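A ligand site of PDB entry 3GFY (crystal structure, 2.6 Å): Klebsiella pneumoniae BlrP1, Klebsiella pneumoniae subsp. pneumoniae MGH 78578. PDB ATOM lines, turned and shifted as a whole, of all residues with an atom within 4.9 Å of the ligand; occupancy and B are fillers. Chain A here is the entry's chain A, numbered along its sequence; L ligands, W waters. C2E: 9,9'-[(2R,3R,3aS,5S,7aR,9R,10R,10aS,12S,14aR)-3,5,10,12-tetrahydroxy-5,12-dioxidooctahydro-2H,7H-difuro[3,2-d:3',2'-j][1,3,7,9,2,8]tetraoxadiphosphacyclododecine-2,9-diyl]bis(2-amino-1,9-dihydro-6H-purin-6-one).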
ATOM      1  N   PHE A 179     -14.476 -28.553  20.354  1.00  0.00           N
ATOM      2  CA  PHE A 179     -13.950 -27.202  20.537  1.00  0.00           C
ATOM      3  C   PHE A 179     -12.676 -26.970  19.763  1.00  0.00           C
ATOM      4  O   PHE A 179     -11.728 -27.750  19.871  1.00  0.00           O
ATOM      5  CB  PHE A 179     -13.727 -26.897  22.020  1.00  0.00           C
ATOM      6  CG  PHE A 179     -14.959 -26.468  22.748  1.00  0.00           C
ATOM      7  CD1 PHE A 179     -15.739 -27.403  23.428  1.00  0.00           C
ATOM      8  CD2 PHE A 179     -15.356 -25.132  22.754  1.00  0.00           C
ATOM      9  CE1 PHE A 179     -16.888 -27.015  24.099  1.00  0.00           C
ATOM     10  CE2 PHE A 179     -16.505 -24.744  23.424  1.00  0.00           C
ATOM     11  CZ  PHE A 179     -17.271 -25.682  24.106  1.00  0.00           C
ATOM     12  N   GLN A 182      -8.032 -21.283  19.581  1.00  0.00           N
ATOM     13  CA  GLN A 182      -7.251 -20.241  18.931  1.00  0.00           C
ATOM     14  C   GLN A 182      -6.418 -19.479  19.961  1.00  0.00           C
ATOM     15  O   GLN A 182      -6.936 -19.022  20.978  1.00  0.00           O
ATOM     16  CB  GLN A 182      -8.147 -19.268  18.152  1.00  0.00           C
ATOM     17  CG  GLN A 182      -7.367 -18.184  17.417  1.00  0.00           C
ATOM     18  CD  GLN A 182      -8.220 -17.404  16.428  1.00  0.00           C
ATOM     19  OE1 GLN A 182      -9.388 -17.120  16.685  1.00  0.00           O
ATOM     20  NE2 GLN A 182      -7.637 -17.056  15.291  1.00  0.00           N
ATOM     21  N   GLU A 196      -8.562 -19.278  23.165  1.00  0.00           N
ATOM     22  CA  GLU A 196     -10.005 -19.174  23.094  1.00  0.00           C
ATOM     23  C   GLU A 196     -10.657 -20.467  22.623  1.00  0.00           C
ATOM     24  O   GLU A 196     -10.281 -21.013  21.588  1.00  0.00           O
ATOM     25  CB  GLU A 196     -10.466 -18.011  22.215  1.00  0.00           C
ATOM     26  CG  GLU A 196     -11.979 -17.920  22.171  1.00  0.00           C
ATOM     27  CD  GLU A 196     -12.504 -16.751  21.387  1.00  0.00           C
ATOM     28  OE1 GLU A 196     -11.711 -16.101  20.667  1.00  0.00           O
ATOM     29  OE2 GLU A 196     -13.718 -16.479  21.485  1.00  0.00           O
ATOM     30  N   ALA A 197     -11.608 -20.953  23.412  1.00  0.00           N
ATOM     31  CA  ALA A 197     -12.431 -22.097  23.060  1.00  0.00           C
ATOM     32  C   ALA A 197     -13.587 -21.664  22.163  1.00  0.00           C
ATOM     33  O   ALA A 197     -14.368 -20.779  22.524  1.00  0.00           O
ATOM     34  CB  ALA A 197     -12.956 -22.777  24.308  1.00  0.00           C
ATOM     35  N   LEU A 198     -13.673 -22.284  20.992  1.00  0.00           N
ATOM     36  CA  LEU A 198     -14.726 -22.001  20.031  1.00  0.00           C
ATOM     37  C   LEU A 198     -15.480 -23.298  19.756  1.00  0.00           C
ATOM     38  O   LEU A 198     -14.877 -24.288  19.341  1.00  0.00           O
ATOM     39  CB  LEU A 198     -14.112 -21.457  18.744  1.00  0.00           C
ATOM     40  CG  LEU A 198     -13.302 -20.159  18.866  1.00  0.00           C
ATOM     41  CD1 LEU A 198     -12.355 -19.981  17.687  1.00  0.00           C
ATOM     42  CD2 LEU A 198     -14.232 -18.973  19.019  1.00  0.00           C
ATOM     43  N   ILE A 199     -16.790 -23.283  19.976  1.00  0.00           N
ATOM     44  CA  ILE A 199     -17.596 -24.503  19.875  1.00  0.00           C
ATOM     45  C   ILE A 199     -17.686 -25.021  18.432  1.00  0.00           C
ATOM     46  O   ILE A 199     -17.657 -24.246  17.464  1.00  0.00           O
ATOM     47  CB  ILE A 199     -19.002 -24.334  20.518  1.00  0.00           C
ATOM     48  CG1 ILE A 199     -19.566 -25.682  20.976  1.00  0.00           C
ATOM     49  CG2 ILE A 199     -19.968 -23.603  19.581  1.00  0.00           C
ATOM     50  CD1 ILE A 199     -20.791 -25.563  21.860  1.00  0.00           C
ATOM     51  N   ARG A 200     -17.758 -26.338  18.304  1.00  0.00           N
ATOM     52  CA  ARG A 200     -17.868 -26.989  17.015  1.00  0.00           C
ATOM     53  C   ARG A 200     -18.884 -28.116  17.122  1.00  0.00           C
ATOM     54  O   ARG A 200     -19.145 -28.627  18.213  1.00  0.00           O
ATOM     55  CB  ARG A 200     -16.507 -27.537  16.580  1.00  0.00           C
ATOM     56  CG  ARG A 200     -15.425 -26.490  16.301  1.00  0.00           C
ATOM     57  CD  ARG A 200     -15.671 -25.771  14.984  1.00  0.00           C
ATOM     58  NE  ARG A 200     -14.652 -24.768  14.680  1.00  0.00           N
ATOM     59  CZ  ARG A 200     -14.719 -23.485  15.028  1.00  0.00           C
ATOM     60  NH1 ARG A 200     -15.772 -23.031  15.715  1.00  0.00           N
ATOM     61  NH2 ARG A 200     -13.755 -22.654  14.700  1.00  0.00           N
ATOM     62  N   PRO A 207     -20.089 -22.979  14.885  1.00  0.00           N
ATOM     63  CA  PRO A 207     -20.970 -22.740  16.026  1.00  0.00           C
ATOM     64  C   PRO A 207     -22.452 -22.632  15.637  1.00  0.00           C
ATOM     65  O   PRO A 207     -23.315 -23.081  16.389  1.00  0.00           O
ATOM     66  CB  PRO A 207     -20.464 -21.414  16.579  1.00  0.00           C
ATOM     67  CG  PRO A 207     -19.046 -21.379  16.197  1.00  0.00           C
ATOM     68  CD  PRO A 207     -18.993 -21.991  14.839  1.00  0.00           C
ATOM     69  N   PHE A 211     -25.382 -25.173  17.089  1.00  0.00           N
ATOM     70  CA  PHE A 211     -26.563 -24.688  17.826  1.00  0.00           C
ATOM     71  C   PHE A 211     -27.892 -24.905  17.099  1.00  0.00           C
ATOM     72  O   PHE A 211     -28.938 -24.960  17.734  1.00  0.00           O
ATOM     73  CB  PHE A 211     -26.395 -23.218  18.226  1.00  0.00           C
ATOM     74  CG  PHE A 211     -25.628 -23.029  19.514  1.00  0.00           C
ATOM     75  CD1 PHE A 211     -26.268 -23.155  20.739  1.00  0.00           C
ATOM     76  CD2 PHE A 211     -24.279 -22.716  19.491  1.00  0.00           C
ATOM     77  CE1 PHE A 211     -25.567 -22.981  21.924  1.00  0.00           C
ATOM     78  CE2 PHE A 211     -23.570 -22.541  20.665  1.00  0.00           C
ATOM     79  CZ  PHE A 211     -24.218 -22.672  21.892  1.00  0.00           C
ATOM     80  N   ASP A 223     -25.398 -24.518  25.850  1.00  0.00           N
ATOM     81  CA  ASP A 223     -24.270 -23.596  25.811  1.00  0.00           C
ATOM     82  C   ASP A 223     -23.463 -23.644  27.094  1.00  0.00           C
ATOM     83  O   ASP A 223     -22.229 -23.634  27.059  1.00  0.00           O
ATOM     84  CB  ASP A 223     -24.751 -22.168  25.537  1.00  0.00           C
ATOM     85  CG  ASP A 223     -23.601 -21.203  25.316  1.00  0.00           C
ATOM     86  OD1 ASP A 223     -22.555 -21.648  24.811  1.00  0.00           O
ATOM     87  OD2 ASP A 223     -23.752 -20.005  25.645  1.00  0.00           O
ATOM     88  N   SER A 226     -21.974 -27.409  27.596  1.00  0.00           N
ATOM     89  CA  SER A 226     -20.939 -27.729  26.612  1.00  0.00           C
ATOM     90  C   SER A 226     -19.552 -27.320  27.103  1.00  0.00           C
ATOM     91  O   SER A 226     -18.547 -27.795  26.599  1.00  0.00           O
ATOM     92  CB  SER A 226     -21.227 -27.048  25.278  1.00  0.00           C
ATOM     93  OG  SER A 226     -21.123 -25.640  25.378  1.00  0.00           O
ATOM     94  N   LYS A 227     -19.517 -26.440  28.106  1.00  0.00           N
ATOM     95  CA  LYS A 227     -18.257 -25.916  28.622  1.00  0.00           C
ATOM     96  C   LYS A 227     -17.435 -26.952  29.384  1.00  0.00           C
ATOM     97  O   LYS A 227     -16.228 -26.804  29.529  1.00  0.00           O
ATOM     98  CB  LYS A 227     -18.502 -24.672  29.486  1.00  0.00           C
ATOM     99  CG  LYS A 227     -19.071 -23.504  28.713  1.00  0.00           C
ATOM    100  CD  LYS A 227     -18.316 -23.325  27.412  1.00  0.00           C
ATOM    101  CE  LYS A 227     -18.883 -22.234  26.552  1.00  0.00           C
ATOM    102  NZ  LYS A 227     -20.008 -22.674  25.695  1.00  0.00           N
ATOM    103  N   ASN A 247     -16.735 -18.604  25.623  1.00  0.00           N
ATOM    104  CA  ASN A 247     -17.802 -17.624  25.362  1.00  0.00           C
ATOM    105  C   ASN A 247     -19.116 -18.150  25.925  1.00  0.00           C
ATOM    106  O   ASN A 247     -19.376 -19.353  25.865  1.00  0.00           O
ATOM    107  CB  ASN A 247     -18.019 -17.471  23.854  1.00  0.00           C
ATOM    108  CG  ASN A 247     -16.779 -17.038  23.113  1.00  0.00           C
ATOM    109  OD1 ASN A 247     -16.499 -15.843  23.001  1.00  0.00           O
ATOM    110  ND2 ASN A 247     -16.040 -18.009  22.571  1.00  0.00           N
ATOM    111  N   LEU A 248     -19.967 -17.264  26.437  1.00  0.00           N
ATOM    112  CA  LEU A 248     -21.285 -17.674  26.939  1.00  0.00           C
ATOM    113  C   LEU A 248     -22.372 -16.643  26.677  1.00  0.00           C
ATOM    114  O   LEU A 248     -22.142 -15.441  26.758  1.00  0.00           O
ATOM    115  CB  LEU A 248     -21.231 -17.993  28.440  1.00  0.00           C
ATOM    116  CG  LEU A 248     -20.788 -19.367  28.930  1.00  0.00           C
ATOM    117  CD1 LEU A 248     -20.660 -19.360  30.443  1.00  0.00           C
ATOM    118  CD2 LEU A 248     -21.742 -20.478  28.486  1.00  0.00           C
ATOM    119  N   LEU A 249     -23.572 -17.142  26.358  1.00  0.00           N
ATOM    120  CA  LEU A 249     -24.770 -16.297  26.285  1.00  0.00           C
ATOM    121  C   LEU A 249     -25.186 -15.890  27.706  1.00  0.00           C
ATOM    122  O   LEU A 249     -25.021 -16.680  28.639  1.00  0.00           O
ATOM    123  CB  LEU A 249     -25.918 -17.047  25.606  1.00  0.00           C
ATOM    124  CG  LEU A 249     -25.805 -17.373  24.103  1.00  0.00           C
ATOM    125  CD1 LEU A 249     -26.779 -18.483  23.724  1.00  0.00           C
ATOM    126  CD2 LEU A 249     -26.017 -16.137  23.238  1.00  0.00           C
ATOM    127  N   GLU A 280     -16.412 -14.833  28.090  1.00  0.00           N
ATOM    128  CA  GLU A 280     -16.681 -13.788  27.101  1.00  0.00           C
ATOM    129  C   GLU A 280     -18.178 -13.622  26.839  1.00  0.00           C
ATOM    130  O   GLU A 280     -18.936 -14.598  26.818  1.00  0.00           O
ATOM    131  CB  GLU A 280     -15.927 -14.050  25.794  1.00  0.00           C
ATOM    132  CG  GLU A 280     -14.419 -13.829  25.921  1.00  0.00           C
ATOM    133  CD  GLU A 280     -13.639 -13.980  24.611  1.00  0.00           C
ATOM    134  OE1 GLU A 280     -12.391 -13.933  24.668  1.00  0.00           O
ATOM    135  OE2 GLU A 280     -14.256 -14.165  23.529  1.00  0.00           O
ATOM    136  N   ASP A 310     -16.913  -9.219  24.476  1.00  0.00           N
ATOM    137  CA  ASP A 310     -16.529  -9.726  23.152  1.00  0.00           C
ATOM    138  C   ASP A 310     -17.188  -8.919  22.044  1.00  0.00           C
ATOM    139  O   ASP A 310     -18.295  -8.404  22.213  1.00  0.00           O
ATOM    140  CB  ASP A 310     -16.903 -11.214  23.030  1.00  0.00           C
ATOM    141  CG  ASP A 310     -16.075 -11.944  21.981  1.00  0.00           C
ATOM    142  OD1 ASP A 310     -15.099 -11.343  21.470  1.00  0.00           O
ATOM    143  OD2 ASP A 310     -16.396 -13.114  21.678  1.00  0.00           O
ATOM    144  N   GLU A 367      -8.906  -8.376  17.774  1.00  0.00           N
ATOM    145  CA  GLU A 367      -9.423  -9.566  17.096  1.00  0.00           C
ATOM    146  C   GLU A 367      -9.365  -9.447  15.585  1.00  0.00           C
ATOM    147  O   GLU A 367      -9.373  -8.344  15.031  1.00  0.00           O
ATOM    148  CB  GLU A 367     -10.893  -9.789  17.472  1.00  0.00           C
ATOM    149  CG  GLU A 367     -11.136 -10.461  18.796  1.00  0.00           C
ATOM    150  CD  GLU A 367     -12.598 -10.824  18.960  1.00  0.00           C
ATOM    151  OE1 GLU A 367     -12.991 -11.935  18.522  1.00  0.00           O
ATOM    152  OE2 GLU A 367     -13.359  -9.988  19.506  1.00  0.00           O
ATOM    153  N   GLY A 368      -9.352 -10.605  14.920  1.00  0.00           N
ATOM    154  CA  GLY A 368      -9.487 -10.676  13.457  1.00  0.00           C
ATOM    155  C   GLY A 368      -8.316 -10.108  12.689  1.00  0.00           C
ATOM    156  O   GLY A 368      -8.490  -9.584  11.588  1.00  0.00           O
ATOM    157  N   VAL A 369      -7.117 -10.227  13.265  1.00  0.00           N
ATOM    158  CA  VAL A 369      -5.914  -9.711  12.628  1.00  0.00           C
ATOM    159  C   VAL A 369      -5.462 -10.686  11.541  1.00  0.00           C
ATOM    160  O   VAL A 369      -5.039 -11.804  11.833  1.00  0.00           O
ATOM    161  CB  VAL A 369      -4.770  -9.464  13.645  1.00  0.00           C
ATOM    162  CG1 VAL A 369      -3.633  -8.705  12.979  1.00  0.00           C
ATOM    163  CG2 VAL A 369      -5.286  -8.684  14.849  1.00  0.00           C
ATOM    164  N   GLU A 370      -5.588 -10.240  10.300  1.00  0.00           N
ATOM    165  CA  GLU A 370      -5.326 -11.095   9.147  1.00  0.00           C
ATOM    166  C   GLU A 370      -4.009 -10.748   8.444  1.00  0.00           C
ATOM    167  O   GLU A 370      -3.380 -11.625   7.849  1.00  0.00           O
ATOM    168  CB  GLU A 370      -6.487 -10.998   8.156  1.00  0.00           C
ATOM    169  CG  GLU A 370      -7.784 -11.644   8.630  1.00  0.00           C
ATOM    170  CD  GLU A 370      -8.953 -11.401   7.684  1.00  0.00           C
ATOM    171  OE1 GLU A 370      -8.817 -10.567   6.757  1.00  0.00           O
ATOM    172  OE2 GLU A 370     -10.008 -12.032   7.870  1.00  0.00           O
ATOM    173  N   GLN A 387      -5.210 -11.571  18.215  1.00  0.00           N
ATOM    174  CA  GLN A 387      -5.879 -12.802  17.826  1.00  0.00           C
ATOM    175  C   GLN A 387      -6.233 -12.725  16.350  1.00  0.00           C
ATOM    176  O   GLN A 387      -6.801 -11.734  15.894  1.00  0.00           O
ATOM    177  CB  GLN A 387      -7.134 -13.020  18.659  1.00  0.00           C
ATOM    178  CG  GLN A 387      -7.819 -14.354  18.424  1.00  0.00           C
ATOM    179  CD  GLN A 387      -9.014 -14.564  19.320  1.00  0.00           C
ATOM    180  OE1 GLN A 387      -9.203 -13.837  20.300  1.00  0.00           O
ATOM    181  NE2 GLN A 387      -9.834 -15.548  18.997  1.00  0.00           N
ATOM    182  N   GLY A 388      -5.884 -13.760  15.603  1.00  0.00           N
ATOM    183  CA  GLY A 388      -6.237 -13.810  14.194  1.00  0.00           C
ATOM    184  C   GLY A 388      -5.540 -14.869  13.374  1.00  0.00           C
ATOM    185  O   GLY A 388      -4.631 -15.568  13.849  1.00  0.00           O
ATOM    186  N   PHE A 389      -5.964 -14.972  12.117  1.00  0.00           N
ATOM    187  CA  PHE A 389      -5.462 -15.964  11.179  1.00  0.00           C
ATOM    188  C   PHE A 389      -3.989 -15.720  10.816  1.00  0.00           C
ATOM    189  O   PHE A 389      -3.274 -16.651  10.464  1.00  0.00           O
ATOM    190  CB  PHE A 389      -6.312 -15.995   9.908  1.00  0.00           C
ATOM    191  CG  PHE A 389      -7.719 -16.524  10.112  1.00  0.00           C
ATOM    192  CD1 PHE A 389      -8.048 -17.295  11.238  1.00  0.00           C
ATOM    193  CD2 PHE A 389      -8.696 -16.300   9.155  1.00  0.00           C
ATOM    194  CE1 PHE A 389      -9.338 -17.788  11.417  1.00  0.00           C
ATOM    195  CE2 PHE A 389      -9.986 -16.801   9.315  1.00  0.00           C
ATOM    196  CZ  PHE A 389     -10.304 -17.547  10.452  1.00  0.00           C
ATOM    197  N   LEU A 390      -3.553 -14.467  10.931  1.00  0.00           N
ATOM    198  CA  LEU A 390      -2.152 -14.107  10.714  1.00  0.00           C
ATOM    199  C   LEU A 390      -1.227 -14.864  11.661  1.00  0.00           C
ATOM    200  O   LEU A 390      -0.136 -15.297  11.260  1.00  0.00           O
ATOM    201  CB  LEU A 390      -1.964 -12.594  10.878  1.00  0.00           C
ATOM    202  CG  LEU A 390      -0.560 -12.052  10.559  1.00  0.00           C
ATOM    203  CD1 LEU A 390      -0.323 -12.020   9.054  1.00  0.00           C
ATOM    204  CD2 LEU A 390      -0.360 -10.676  11.174  1.00  0.00           C
ATOM    205  N   PRO A 394      -7.728 -21.378  14.307  1.00  0.00           N
ATOM    206  CA  PRO A 394      -8.410 -22.279  15.257  1.00  0.00           C
ATOM    207  C   PRO A 394      -8.157 -23.740  14.912  1.00  0.00           C
ATOM    208  O   PRO A 394      -8.236 -24.138  13.754  1.00  0.00           O
ATOM    209  CB  PRO A 394      -9.890 -21.943  15.053  1.00  0.00           C
ATOM    210  CG  PRO A 394      -9.890 -20.544  14.556  1.00  0.00           C
ATOM    211  CD  PRO A 394      -8.663 -20.421  13.709  1.00  0.00           C
HETATM  212  P1  C2E L   1     -15.702 -14.538  18.499  1.00  0.00           P
HETATM  213  O2P C2E L   1     -15.364 -15.241  19.788  1.00  0.00           O
HETATM  214  O1P C2E L   1     -15.971 -13.055  18.562  1.00  0.00           O
HETATM  215  O5' C2E L   1     -14.490 -14.682  17.462  1.00  0.00           O
HETATM  216  C5' C2E L   1     -13.894 -15.912  17.086  1.00  0.00           C
HETATM  217  C4' C2E L   1     -14.277 -16.164  15.632  1.00  0.00           C
HETATM  218  O4' C2E L   1     -13.537 -15.301  14.765  1.00  0.00           O
HETATM  219  C3' C2E L   1     -13.911 -17.580  15.225  1.00  0.00           C
HETATM  220  O3' C2E L   1     -14.949 -18.058  14.375  1.00  0.00           O
HETATM  221  C2' C2E L   1     -12.693 -17.417  14.393  1.00  0.00           C
HETATM  222  O2' C2E L   1     -12.330 -18.404  13.582  1.00  0.00           O
HETATM  223  C1' C2E L   1     -12.616 -16.146  14.018  1.00  0.00           C
HETATM  224  N9  C2E L   1     -11.434 -15.578  13.653  1.00  0.00           N
HETATM  225  C8  C2E L   1     -10.376 -15.610  14.365  1.00  0.00           C
HETATM  226  N7  C2E L   1      -9.464 -14.976  13.739  1.00  0.00           N
HETATM  227  C5  C2E L   1      -9.934 -14.494  12.567  1.00  0.00           C
HETATM  228  C6  C2E L   1      -9.408 -13.751  11.520  1.00  0.00           C
HETATM  229  O6  C2E L   1      -8.219 -13.377  11.545  1.00  0.00           O
HETATM  230  N1  C2E L   1     -10.215 -13.450  10.477  1.00  0.00           N
HETATM  231  C2  C2E L   1     -11.503 -13.858  10.455  1.00  0.00           C
HETATM  232  N2  C2E L   1     -12.276 -13.540   9.394  1.00  0.00           N
HETATM  233  N3  C2E L   1     -12.043 -14.577  11.458  1.00  0.00           N
HETATM  234  C4  C2E L   1     -11.265 -14.902  12.523  1.00  0.00           C
HETATM  235  P11 C2E L   1     -16.083 -19.002  14.979  1.00  0.00           P
HETATM  236  O21 C2E L   1     -16.668 -19.839  13.745  1.00  0.00           O
HETATM  237  O11 C2E L   1     -15.363 -20.090  15.916  1.00  0.00           O
HETATM  238  O5A C2E L   1     -17.013 -18.191  16.025  1.00  0.00           O
HETATM  239  C5A C2E L   1     -18.248 -17.574  15.679  1.00  0.00           C
HETATM  240  C4A C2E L   1     -18.579 -16.915  17.014  1.00  0.00           C
HETATM  241  O4A C2E L   1     -19.464 -17.746  17.779  1.00  0.00           O
HETATM  242  C3A C2E L   1     -17.400 -16.589  17.942  1.00  0.00           C
HETATM  243  O3A C2E L   1     -16.953 -15.243  17.767  1.00  0.00           O
HETATM  244  C2A C2E L   1     -17.994 -16.806  19.305  1.00  0.00           C
HETATM  245  O2A C2E L   1     -18.737 -15.754  19.616  1.00  0.00           O
HETATM  246  C1A C2E L   1     -18.786 -17.844  19.050  1.00  0.00           C
HETATM  247  N91 C2E L   1     -18.804 -18.929  19.868  1.00  0.00           N
HETATM  248  C81 C2E L   1     -17.848 -19.844  19.773  1.00  0.00           C
HETATM  249  N71 C2E L   1     -18.135 -20.756  20.721  1.00  0.00           N
HETATM  250  C51 C2E L   1     -19.254 -20.364  21.379  1.00  0.00           C
HETATM  251  C61 C2E L   1     -19.958 -20.920  22.430  1.00  0.00           C
HETATM  252  O61 C2E L   1     -19.575 -21.997  22.944  1.00  0.00           O
HETATM  253  N11 C2E L   1     -21.062 -20.289  22.886  1.00  0.00           N
HETATM  254  C21 C2E L   1     -21.480 -19.125  22.356  1.00  0.00           C
HETATM  255  N21 C2E L   1     -22.589 -18.545  22.856  1.00  0.00           N
HETATM  256  N31 C2E L   1     -20.804 -18.557  21.321  1.00  0.00           N
HETATM  257  C41 C2E L   1     -19.691 -19.158  20.830  1.00  0.00           C
HETATM  258  O   HOH W   1     -16.818 -21.763  11.863  1.00  0.00           O
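An oxygen (O2P) of the ligand lies close to the side-chain carboxylate of Glu 196.
The side-chain carboxylate (OD1) of Asp 223 lies within hydrogen-bond range of a nitrogen (N11) of the ligand (2.8 Å).
The backbone NH of Phe 389 sits at hydrogen-bond distance from an oxygen (O6) of the ligand (2.8 Å).
O61 of the ligand sits at hydrogen-bond distance from NZ of Lys 227, 2.9 Å away.
A nitrogen (N7) of the ligand sits at hydrogen-bond distance from the side-chain amide nitrogen (NE2) of Gln 182.
N71 of the ligand is in hydrogen-bond range of N of Ile 199 (3.0 Å).
N1 of the ligand lies within hydrogen-bond range of OE2 of Glu 370 (3.0 Å).
An oxygen (O11) of the ligand is in salt-bridge range of the guanidinium group of Arg 200, at 3.0 Å.
The side-chain carboxylate (OD2) of Asp 310 sits close to an oxygen (O2P) of the ligand (3.0 Å).
An oxygen (O2P) of the ligand lies close to the side-chain amide oxygen (OD1) of Asn 247 (3.5 Å).
The side-chain carboxylate (OE2) of Glu 196 lies within hydrogen-bond range of the side-chain amide nitrogen (ND2) of Asn 247, at 3.0 Å.
OE1 of Glu 196 lies within hydrogen-bond range of NE2 of Gln 387, at 2.6 Å.
The side-chain carboxylate (OD2) of Asp 223 lies within hydrogen-bond range of the backbone NH (N) of Leu 249 (3.0 Å).
The backbone carbonyl oxygen (O) of Asp 223 lies within hydrogen-bond range of the side-chain hydroxyl (OG) of Ser 226 (2.8 Å).
The side-chain amino group (NZ) of Lys 227 lies close to the backbone carbonyl oxygen (O) of Asn 247 (3.4 Å).
NZ of Lys 227 is in hydrogen-bond range of OG of Ser 226, 3.2 Å away.
NE2 of Gln 387 is in hydrogen-bond range of OE1 of Gln 182, at 2.8 Å.
The backbone NH of Val 369 sits at hydrogen-bond distance from the backbone carbonyl oxygen of Gln 387 (3.0 Å).
The side-chain carboxylate (OE1) of Glu 367 lies close to an oxygen (O1P) of the ligand (3.2 Å).
Merely in contact with the ligand: Gly 388 (3.3 Å), Pro 207 (3.4 Å), Leu 198 (3.4 Å), Pro 394 (3.4 Å), Gly 368 (3.5 Å), Val 369 (3.6 Å) and Leu 249 (3.6 Å).
Hydrophobic or aromatic side chains within 4 Å of the ligand: Leu 198, Ile 199, Pro 207, Leu 249, Phe 389 and Pro 394.
Within 4 Å of the ligand: Gln 182, Glu 196, Leu 198, Ile 199, Arg 200, Pro 207, Asp 223, Lys 227, Asn 247, Leu 249, Asp 310, Glu 367, Gly 368, Val 369, Glu 370, Gly 388, Phe 389 and Pro 394.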
